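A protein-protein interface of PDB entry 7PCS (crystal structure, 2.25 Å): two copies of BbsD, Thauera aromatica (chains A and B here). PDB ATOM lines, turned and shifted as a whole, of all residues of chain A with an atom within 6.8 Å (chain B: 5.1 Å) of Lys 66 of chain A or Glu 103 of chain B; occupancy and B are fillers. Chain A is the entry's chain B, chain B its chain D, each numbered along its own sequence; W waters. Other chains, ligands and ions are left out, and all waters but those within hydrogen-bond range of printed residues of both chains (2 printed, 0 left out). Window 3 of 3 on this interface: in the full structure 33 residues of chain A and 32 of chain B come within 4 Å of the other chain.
NZ of Lys 115 of chain A lies within salt-bridge range of OE2 of Glu 103 of chain B (2.9 Å).
OD1 of Asp 107 of chain B lies within salt-bridge range of NZ of Lys 115 of chain A (2.9 Å).
The side-chain amide nitrogen of Gln 122 of chain A lies within hydrogen-bond range of the backbone carbonyl oxygen of Leu 101 of chain B (2.8 Å).
Among the printed residues, merely in contact across the chains: Lys 66 of chain A with Glu 103 of chain B, Lys 115 of chain A with Trp 106 of chain B and Phe 118 of chain A with Trp 106 of chain B.
Lys 66 of chain A touches just one residue of chain B: Glu 103.
Ala 67 of chain A touches none of the printed residues of chain B.
Of the printed residues of chain B, Lys 115 of chain A touches Glu 103 (2.9 Å), Trp 106 (3.4 Å) and Asp 107 (2.9 Å).
Printed residues of chain B within 4 Å of Gln 122 of chain A: Leu 101.
Printed residues of chain A within 4 Å of Leu 101 of chain B: Gln 122 (2.8 Å).
Glu 103 of chain B touches two residues of chain A.
Of the printed residues of chain A, Trp 106 of chain B touches Lys 115 and Phe 118.
Of the printed residues of chain A, Asp 107 of chain B touches Lys 115.
The nearest residue of chain B that does not touch Lys 66 of chain A is Leu 101 of chain B (4.5 Å).
Hydrophobic or aromatic side chains of chain A that line the printed part of chain B: Phe 118.
Of the 7 printed residues of chain B, 4 touch a printed residue of chain A.
Printed residues of chain B that touch a printed residue of chain A: Leu 101, Glu 103, Trp 106 and Asp 107.
Hydrophobic or aromatic side chains of chain B within 4 Å of the printed part of chain A: Leu 101 and Trp 106.
Among the printed residues, Asp or Glu carboxylates within 4 Å of a Lys or Arg side-chain nitrogen of the other chain: Lys 115 of chain A with Glu 103 of chain B (2.9 Å) and Lys 115 of chain A with Asp 107 of chain B (2.9 Å).
No position is printed for both chains.
Of the 6 pairs that touch across the chains among the printed residues, none has its exchanged pair printed and touching as well.
Water W2 lies within hydrogen-bond range of OE1 of Gln 122 of chain A (2.6 Å), NZ of Lys 66 of chain A (2.7 Å), N of Glu 103 of chain B (3.2 Å) and O of Leu 101 of chain B (3.2 Å).
Water W1 bridges the side-chain carboxylate of Glu 103 of chain B and the backbone NH of Lys 66 of chain A.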
ATOM      1  N   ASP A  62     -17.256 -21.739   6.909  1.00  0.00           N
ATOM      2  CA  ASP A  62     -16.877 -21.827   5.500  1.00  0.00           C
ATOM      3  C   ASP A  62     -18.056 -22.438   4.760  1.00  0.00           C
ATOM      4  O   ASP A  62     -18.280 -23.646   4.829  1.00  0.00           O
ATOM      5  CB  ASP A  62     -15.615 -22.670   5.335  1.00  0.00           C
ATOM      6  CG  ASP A  62     -15.252 -22.910   3.876  1.00  0.00           C
ATOM      7  OD1 ASP A  62     -15.907 -22.334   2.983  1.00  0.00           O
ATOM      8  OD2 ASP A  62     -14.319 -23.694   3.618  1.00  0.00           O
ATOM      9  N   ILE A  63     -18.824 -21.607   4.052  1.00  0.00           N
ATOM     10  CA  ILE A  63     -20.006 -22.077   3.347  1.00  0.00           C
ATOM     11  C   ILE A  63     -19.665 -23.077   2.263  1.00  0.00           C
ATOM     12  O   ILE A  63     -20.568 -23.701   1.703  1.00  0.00           O
ATOM     13  CB  ILE A  63     -20.807 -20.878   2.804  1.00  0.00           C
ATOM     14  CG1 ILE A  63     -20.006 -20.067   1.792  1.00  0.00           C
ATOM     15  CG2 ILE A  63     -21.238 -19.983   3.975  1.00  0.00           C
ATOM     16  CD1 ILE A  63     -20.303 -20.465   0.358  1.00  0.00           C
ATOM     17  N   GLY A  64     -18.391 -23.215   1.926  1.00  0.00           N
ATOM     18  CA  GLY A  64     -17.951 -24.260   1.030  1.00  0.00           C
ATOM     19  C   GLY A  64     -17.742 -25.616   1.668  1.00  0.00           C
ATOM     20  O   GLY A  64     -17.438 -26.586   0.967  1.00  0.00           O
ATOM     21  N   ASN A  65     -17.890 -25.709   2.985  1.00  0.00           N
ATOM     22  CA  ASN A  65     -17.698 -26.950   3.726  1.00  0.00           C
ATOM     23  C   ASN A  65     -19.047 -27.396   4.269  1.00  0.00           C
ATOM     24  O   ASN A  65     -19.701 -26.640   4.993  1.00  0.00           O
ATOM     25  CB  ASN A  65     -16.705 -26.757   4.868  1.00  0.00           C
ATOM     26  CG  ASN A  65     -16.394 -28.060   5.600  1.00  0.00           C
ATOM     27  OD1 ASN A  65     -17.209 -28.579   6.375  1.00  0.00           O
ATOM     28  ND2 ASN A  65     -15.200 -28.585   5.366  1.00  0.00           N
ATOM     29  N   LYS A  66     -19.460 -28.623   3.933  1.00  0.00           N
ATOM     30  CA  LYS A  66     -20.818 -29.044   4.272  1.00  0.00           C
ATOM     31  C   LYS A  66     -21.026 -29.094   5.782  1.00  0.00           C
ATOM     32  O   LYS A  66     -22.072 -28.664   6.288  1.00  0.00           O
ATOM     33  CB  LYS A  66     -21.144 -30.405   3.653  1.00  0.00           C
ATOM     34  CG  LYS A  66     -22.609 -30.805   3.867  1.00  0.00           C
ATOM     35  CD  LYS A  66     -22.980 -32.107   3.169  1.00  0.00           C
ATOM     36  CE  LYS A  66     -24.458 -32.439   3.417  1.00  0.00           C
ATOM     37  NZ  LYS A  66     -24.932 -33.613   2.613  1.00  0.00           N
ATOM     38  N   ALA A  67     -20.051 -29.632   6.516  1.00  0.00           N
ATOM     39  CA  ALA A  67     -20.202 -29.728   7.963  1.00  0.00           C
ATOM     40  C   ALA A  67     -20.329 -28.346   8.589  1.00  0.00           C
ATOM     41  O   ALA A  67     -21.169 -28.131   9.471  1.00  0.00           O
ATOM     42  CB  ALA A  67     -19.019 -30.493   8.566  1.00  0.00           C
ATOM     43  N   ALA A  68     -19.508 -27.393   8.141  1.00  0.00           N
ATOM     44  CA  ALA A  68     -19.608 -26.034   8.664  1.00  0.00           C
ATOM     45  C   ALA A  68     -20.951 -25.411   8.308  1.00  0.00           C
ATOM     46  O   ALA A  68     -21.523 -24.657   9.102  1.00  0.00           O
ATOM     47  CB  ALA A  68     -18.463 -25.171   8.132  1.00  0.00           C
ATOM     48  N   VAL A  69     -21.473 -25.715   7.121  1.00  0.00           N
ATOM     49  CA  VAL A  69     -22.763 -25.160   6.723  1.00  0.00           C
ATOM     50  C   VAL A  69     -23.873 -25.687   7.625  1.00  0.00           C
ATOM     51  O   VAL A  69     -24.749 -24.931   8.069  1.00  0.00           O
ATOM     52  CB  VAL A  69     -23.040 -25.476   5.241  1.00  0.00           C
ATOM     53  CG1 VAL A  69     -24.511 -25.282   4.921  1.00  0.00           C
ATOM     54  CG2 VAL A  69     -22.166 -24.628   4.320  1.00  0.00           C
ATOM     55  N   ASP A  70     -23.861 -26.994   7.908  1.00  0.00           N
ATOM     56  CA  ASP A  70     -24.900 -27.572   8.753  1.00  0.00           C
ATOM     57  C   ASP A  70     -24.873 -26.974  10.152  1.00  0.00           C
ATOM     58  O   ASP A  70     -25.927 -26.734  10.754  1.00  0.00           O
ATOM     59  CB  ASP A  70     -24.744 -29.090   8.823  1.00  0.00           C
ATOM     60  CG  ASP A  70     -25.306 -29.783   7.596  1.00  0.00           C
ATOM     61  OD1 ASP A  70     -26.364 -29.336   7.076  1.00  0.00           O
ATOM     62  OD2 ASP A  70     -24.674 -30.763   7.146  1.00  0.00           O
ATOM     63  N   GLY A  71     -23.675 -26.719  10.681  1.00  0.00           N
ATOM     64  CA  GLY A  71     -23.581 -26.100  11.994  1.00  0.00           C
ATOM     65  C   GLY A  71     -24.114 -24.682  12.002  1.00  0.00           C
ATOM     66  O   GLY A  71     -24.717 -24.241  12.984  1.00  0.00           O
ATOM     67  N   ASN A 111     -16.008 -24.095  -5.728  1.00  0.00           N
ATOM     68  CA  ASN A 111     -16.425 -24.556  -4.408  1.00  0.00           C
ATOM     69  C   ASN A 111     -17.191 -23.472  -3.657  1.00  0.00           C
ATOM     70  O   ASN A 111     -18.280 -23.718  -3.124  1.00  0.00           O
ATOM     71  CB  ASN A 111     -15.191 -25.011  -3.620  1.00  0.00           C
ATOM     72  CG  ASN A 111     -15.546 -25.677  -2.312  1.00  0.00           C
ATOM     73  OD1 ASN A 111     -16.117 -26.774  -2.300  1.00  0.00           O
ATOM     74  ND2 ASN A 111     -15.184 -25.032  -1.194  1.00  0.00           N
ATOM     75  N   LYS A 115     -20.859 -24.699  -5.388  1.00  0.00           N
ATOM     76  CA  LYS A 115     -21.166 -25.709  -4.376  1.00  0.00           C
ATOM     77  C   LYS A 115     -21.643 -25.067  -3.078  1.00  0.00           C
ATOM     78  O   LYS A 115     -22.581 -25.561  -2.438  1.00  0.00           O
ATOM     79  CB  LYS A 115     -19.939 -26.580  -4.105  1.00  0.00           C
ATOM     80  CG  LYS A 115     -20.197 -27.700  -3.109  1.00  0.00           C
ATOM     81  CD  LYS A 115     -18.975 -28.616  -2.945  1.00  0.00           C
ATOM     82  CE  LYS A 115     -19.303 -29.813  -2.054  1.00  0.00           C
ATOM     83  NZ  LYS A 115     -18.116 -30.693  -1.788  1.00  0.00           N
ATOM     84  N   PHE A 118     -25.056 -24.369  -3.352  1.00  0.00           N
ATOM     85  CA  PHE A 118     -25.801 -25.617  -3.273  1.00  0.00           C
ATOM     86  C   PHE A 118     -25.883 -26.121  -1.838  1.00  0.00           C
ATOM     87  O   PHE A 118     -26.943 -26.584  -1.395  1.00  0.00           O
ATOM     88  CB  PHE A 118     -25.154 -26.673  -4.165  1.00  0.00           C
ATOM     89  CG  PHE A 118     -25.596 -28.069  -3.849  1.00  0.00           C
ATOM     90  CD1 PHE A 118     -26.819 -28.545  -4.296  1.00  0.00           C
ATOM     91  CD2 PHE A 118     -24.791 -28.903  -3.101  1.00  0.00           C
ATOM     92  CE1 PHE A 118     -27.225 -29.834  -3.999  1.00  0.00           C
ATOM     93  CE2 PHE A 118     -25.189 -30.191  -2.807  1.00  0.00           C
ATOM     94  CZ  PHE A 118     -26.408 -30.656  -3.254  1.00  0.00           C
ATOM     95  N   LEU A 119     -24.776 -26.044  -1.096  1.00  0.00           N
ATOM     96  CA  LEU A 119     -24.767 -26.576   0.265  1.00  0.00           C
ATOM     97  C   LEU A 119     -25.727 -25.803   1.158  1.00  0.00           C
ATOM     98  O   LEU A 119     -26.493 -26.396   1.924  1.00  0.00           O
ATOM     99  CB  LEU A 119     -23.358 -26.522   0.850  1.00  0.00           C
ATOM    100  CG  LEU A 119     -22.307 -27.458   0.270  1.00  0.00           C
ATOM    101  CD1 LEU A 119     -20.963 -27.204   0.955  1.00  0.00           C
ATOM    102  CD2 LEU A 119     -22.734 -28.897   0.434  1.00  0.00           C
ATOM    103  N   GLN A 122     -29.424 -26.431   0.170  1.00  0.00           N
ATOM    104  CA  GLN A 122     -29.833 -27.753   0.635  1.00  0.00           C
ATOM    105  C   GLN A 122     -30.055 -27.764   2.142  1.00  0.00           C
ATOM    106  O   GLN A 122     -31.073 -28.269   2.633  1.00  0.00           O
ATOM    107  CB  GLN A 122     -28.777 -28.788   0.252  1.00  0.00           C
ATOM    108  CG  GLN A 122     -29.176 -30.214   0.558  1.00  0.00           C
ATOM    109  CD  GLN A 122     -28.052 -31.209   0.292  1.00  0.00           C
ATOM    110  OE1 GLN A 122     -26.881 -30.936   0.561  1.00  0.00           O
ATOM    111  NE2 GLN A 122     -28.408 -32.368  -0.242  1.00  0.00           N
ATOM    112  N   ALA A 123     -29.092 -27.242   2.904  1.00  0.00           N
ATOM    113  CA  ALA A 123     -29.189 -27.335   4.357  1.00  0.00           C
ATOM    114  C   ALA A 123     -30.367 -26.527   4.894  1.00  0.00           C
ATOM    115  O   ALA A 123     -30.929 -26.864   5.942  1.00  0.00           O
ATOM    116  CB  ALA A 123     -27.881 -26.869   4.999  1.00  0.00           C
ATOM    117  N   LEU B 101     -29.968 -35.654  -2.043  1.00  0.00           N
ATOM    118  CA  LEU B 101     -28.725 -35.614  -2.798  1.00  0.00           C
ATOM    119  C   LEU B 101     -27.549 -35.711  -1.834  1.00  0.00           C
ATOM    120  O   LEU B 101     -27.379 -34.848  -0.966  1.00  0.00           O
ATOM    121  CB  LEU B 101     -28.655 -34.326  -3.620  1.00  0.00           C
ATOM    122  CG  LEU B 101     -29.647 -34.242  -4.782  1.00  0.00           C
ATOM    123  CD1 LEU B 101     -29.630 -32.827  -5.396  1.00  0.00           C
ATOM    124  CD2 LEU B 101     -29.357 -35.288  -5.837  1.00  0.00           C
ATOM    125  N   SER B 102     -26.748 -36.761  -1.979  1.00  0.00           N
ATOM    126  CA  SER B 102     -25.532 -36.861  -1.195  1.00  0.00           C
ATOM    127  C   SER B 102     -24.521 -35.828  -1.681  1.00  0.00           C
ATOM    128  O   SER B 102     -24.578 -35.352  -2.819  1.00  0.00           O
ATOM    129  CB  SER B 102     -24.940 -38.264  -1.303  1.00  0.00           C
ATOM    130  OG  SER B 102     -24.444 -38.504  -2.601  1.00  0.00           O
ATOM    131  N   GLU B 103     -23.593 -35.463  -0.794  1.00  0.00           N
ATOM    132  CA  GLU B 103     -22.509 -34.582  -1.213  1.00  0.00           C
ATOM    133  C   GLU B 103     -21.757 -35.174  -2.396  1.00  0.00           C
ATOM    134  O   GLU B 103     -21.241 -34.433  -3.245  1.00  0.00           O
ATOM    135  CB  GLU B 103     -21.557 -34.318  -0.046  1.00  0.00           C
ATOM    136  CG  GLU B 103     -20.534 -33.232  -0.345  1.00  0.00           C
ATOM    137  CD  GLU B 103     -19.645 -32.908   0.843  1.00  0.00           C
ATOM    138  OE1 GLU B 103     -19.765 -33.592   1.876  1.00  0.00           O
ATOM    139  OE2 GLU B 103     -18.811 -31.980   0.735  1.00  0.00           O
ATOM    140  N   ALA B 104     -21.706 -36.507  -2.481  1.00  0.00           N
ATOM    141  CA  ALA B 104     -21.025 -37.169  -3.588  1.00  0.00           C
ATOM    142  C   ALA B 104     -21.842 -37.100  -4.869  1.00  0.00           C
ATOM    143  O   ALA B 104     -21.266 -37.012  -5.959  1.00  0.00           O
ATOM    144  CB  ALA B 104     -20.720 -38.631  -3.238  1.00  0.00           C
ATOM    145  N   ASP B 105     -23.174 -37.154  -4.762  1.00  0.00           N
ATOM    146  CA  ASP B 105     -24.019 -36.954  -5.936  1.00  0.00           C
ATOM    147  C   ASP B 105     -23.705 -35.625  -6.612  1.00  0.00           C
ATOM    148  O   ASP B 105     -23.713 -35.523  -7.846  1.00  0.00           O
ATOM    149  CB  ASP B 105     -25.495 -37.014  -5.535  1.00  0.00           C
ATOM    150  CG  ASP B 105     -25.902 -38.373  -4.996  1.00  0.00           C
ATOM    151  OD1 ASP B 105     -25.274 -39.383  -5.370  1.00  0.00           O
ATOM    152  OD2 ASP B 105     -26.838 -38.433  -4.175  1.00  0.00           O
ATOM    153  N   TRP B 106     -23.437 -34.590  -5.815  1.00  0.00           N
ATOM    154  CA  TRP B 106     -23.110 -33.282  -6.370  1.00  0.00           C
ATOM    155  C   TRP B 106     -21.699 -33.276  -6.944  1.00  0.00           C
ATOM    156  O   TRP B 106     -21.484 -32.882  -8.099  1.00  0.00           O
ATOM    157  CB  TRP B 106     -23.258 -32.204  -5.284  1.00  0.00           C
ATOM    158  CG  TRP B 106     -22.644 -30.897  -5.672  1.00  0.00           C
ATOM    159  CD1 TRP B 106     -21.359 -30.505  -5.454  1.00  0.00           C
ATOM    160  CD2 TRP B 106     -23.286 -29.811  -6.351  1.00  0.00           C
ATOM    161  NE1 TRP B 106     -21.153 -29.247  -5.968  1.00  0.00           N
ATOM    162  CE2 TRP B 106     -22.323 -28.796  -6.518  1.00  0.00           C
ATOM    163  CE3 TRP B 106     -24.580 -29.598  -6.836  1.00  0.00           C
ATOM    164  CZ2 TRP B 106     -22.608 -27.594  -7.155  1.00  0.00           C
ATOM    165  CZ3 TRP B 106     -24.866 -28.400  -7.460  1.00  0.00           C
ATOM    166  CH2 TRP B 106     -23.886 -27.409  -7.608  1.00  0.00           C
ATOM    167  N   ASP B 107     -20.724 -33.718  -6.146  1.00  0.00           N
ATOM    168  CA  ASP B 107     -19.322 -33.573  -6.525  1.00  0.00           C
ATOM    169  C   ASP B 107     -19.024 -34.255  -7.854  1.00  0.00           C
ATOM    170  O   ASP B 107     -18.230 -33.743  -8.653  1.00  0.00           O
ATOM    171  CB  ASP B 107     -18.414 -34.139  -5.427  1.00  0.00           C
ATOM    172  CG  ASP B 107     -18.381 -33.270  -4.188  1.00  0.00           C
ATOM    173  OD1 ASP B 107     -18.673 -32.066  -4.296  1.00  0.00           O
ATOM    174  OD2 ASP B 107     -18.044 -33.782  -3.107  1.00  0.00           O
HETATM  175  O   HOH W   1     -17.726 -30.114   2.307  1.00  0.00           O
HETATM  176  O   HOH W   2     -25.139 -32.765   0.043  1.00  0.00           O
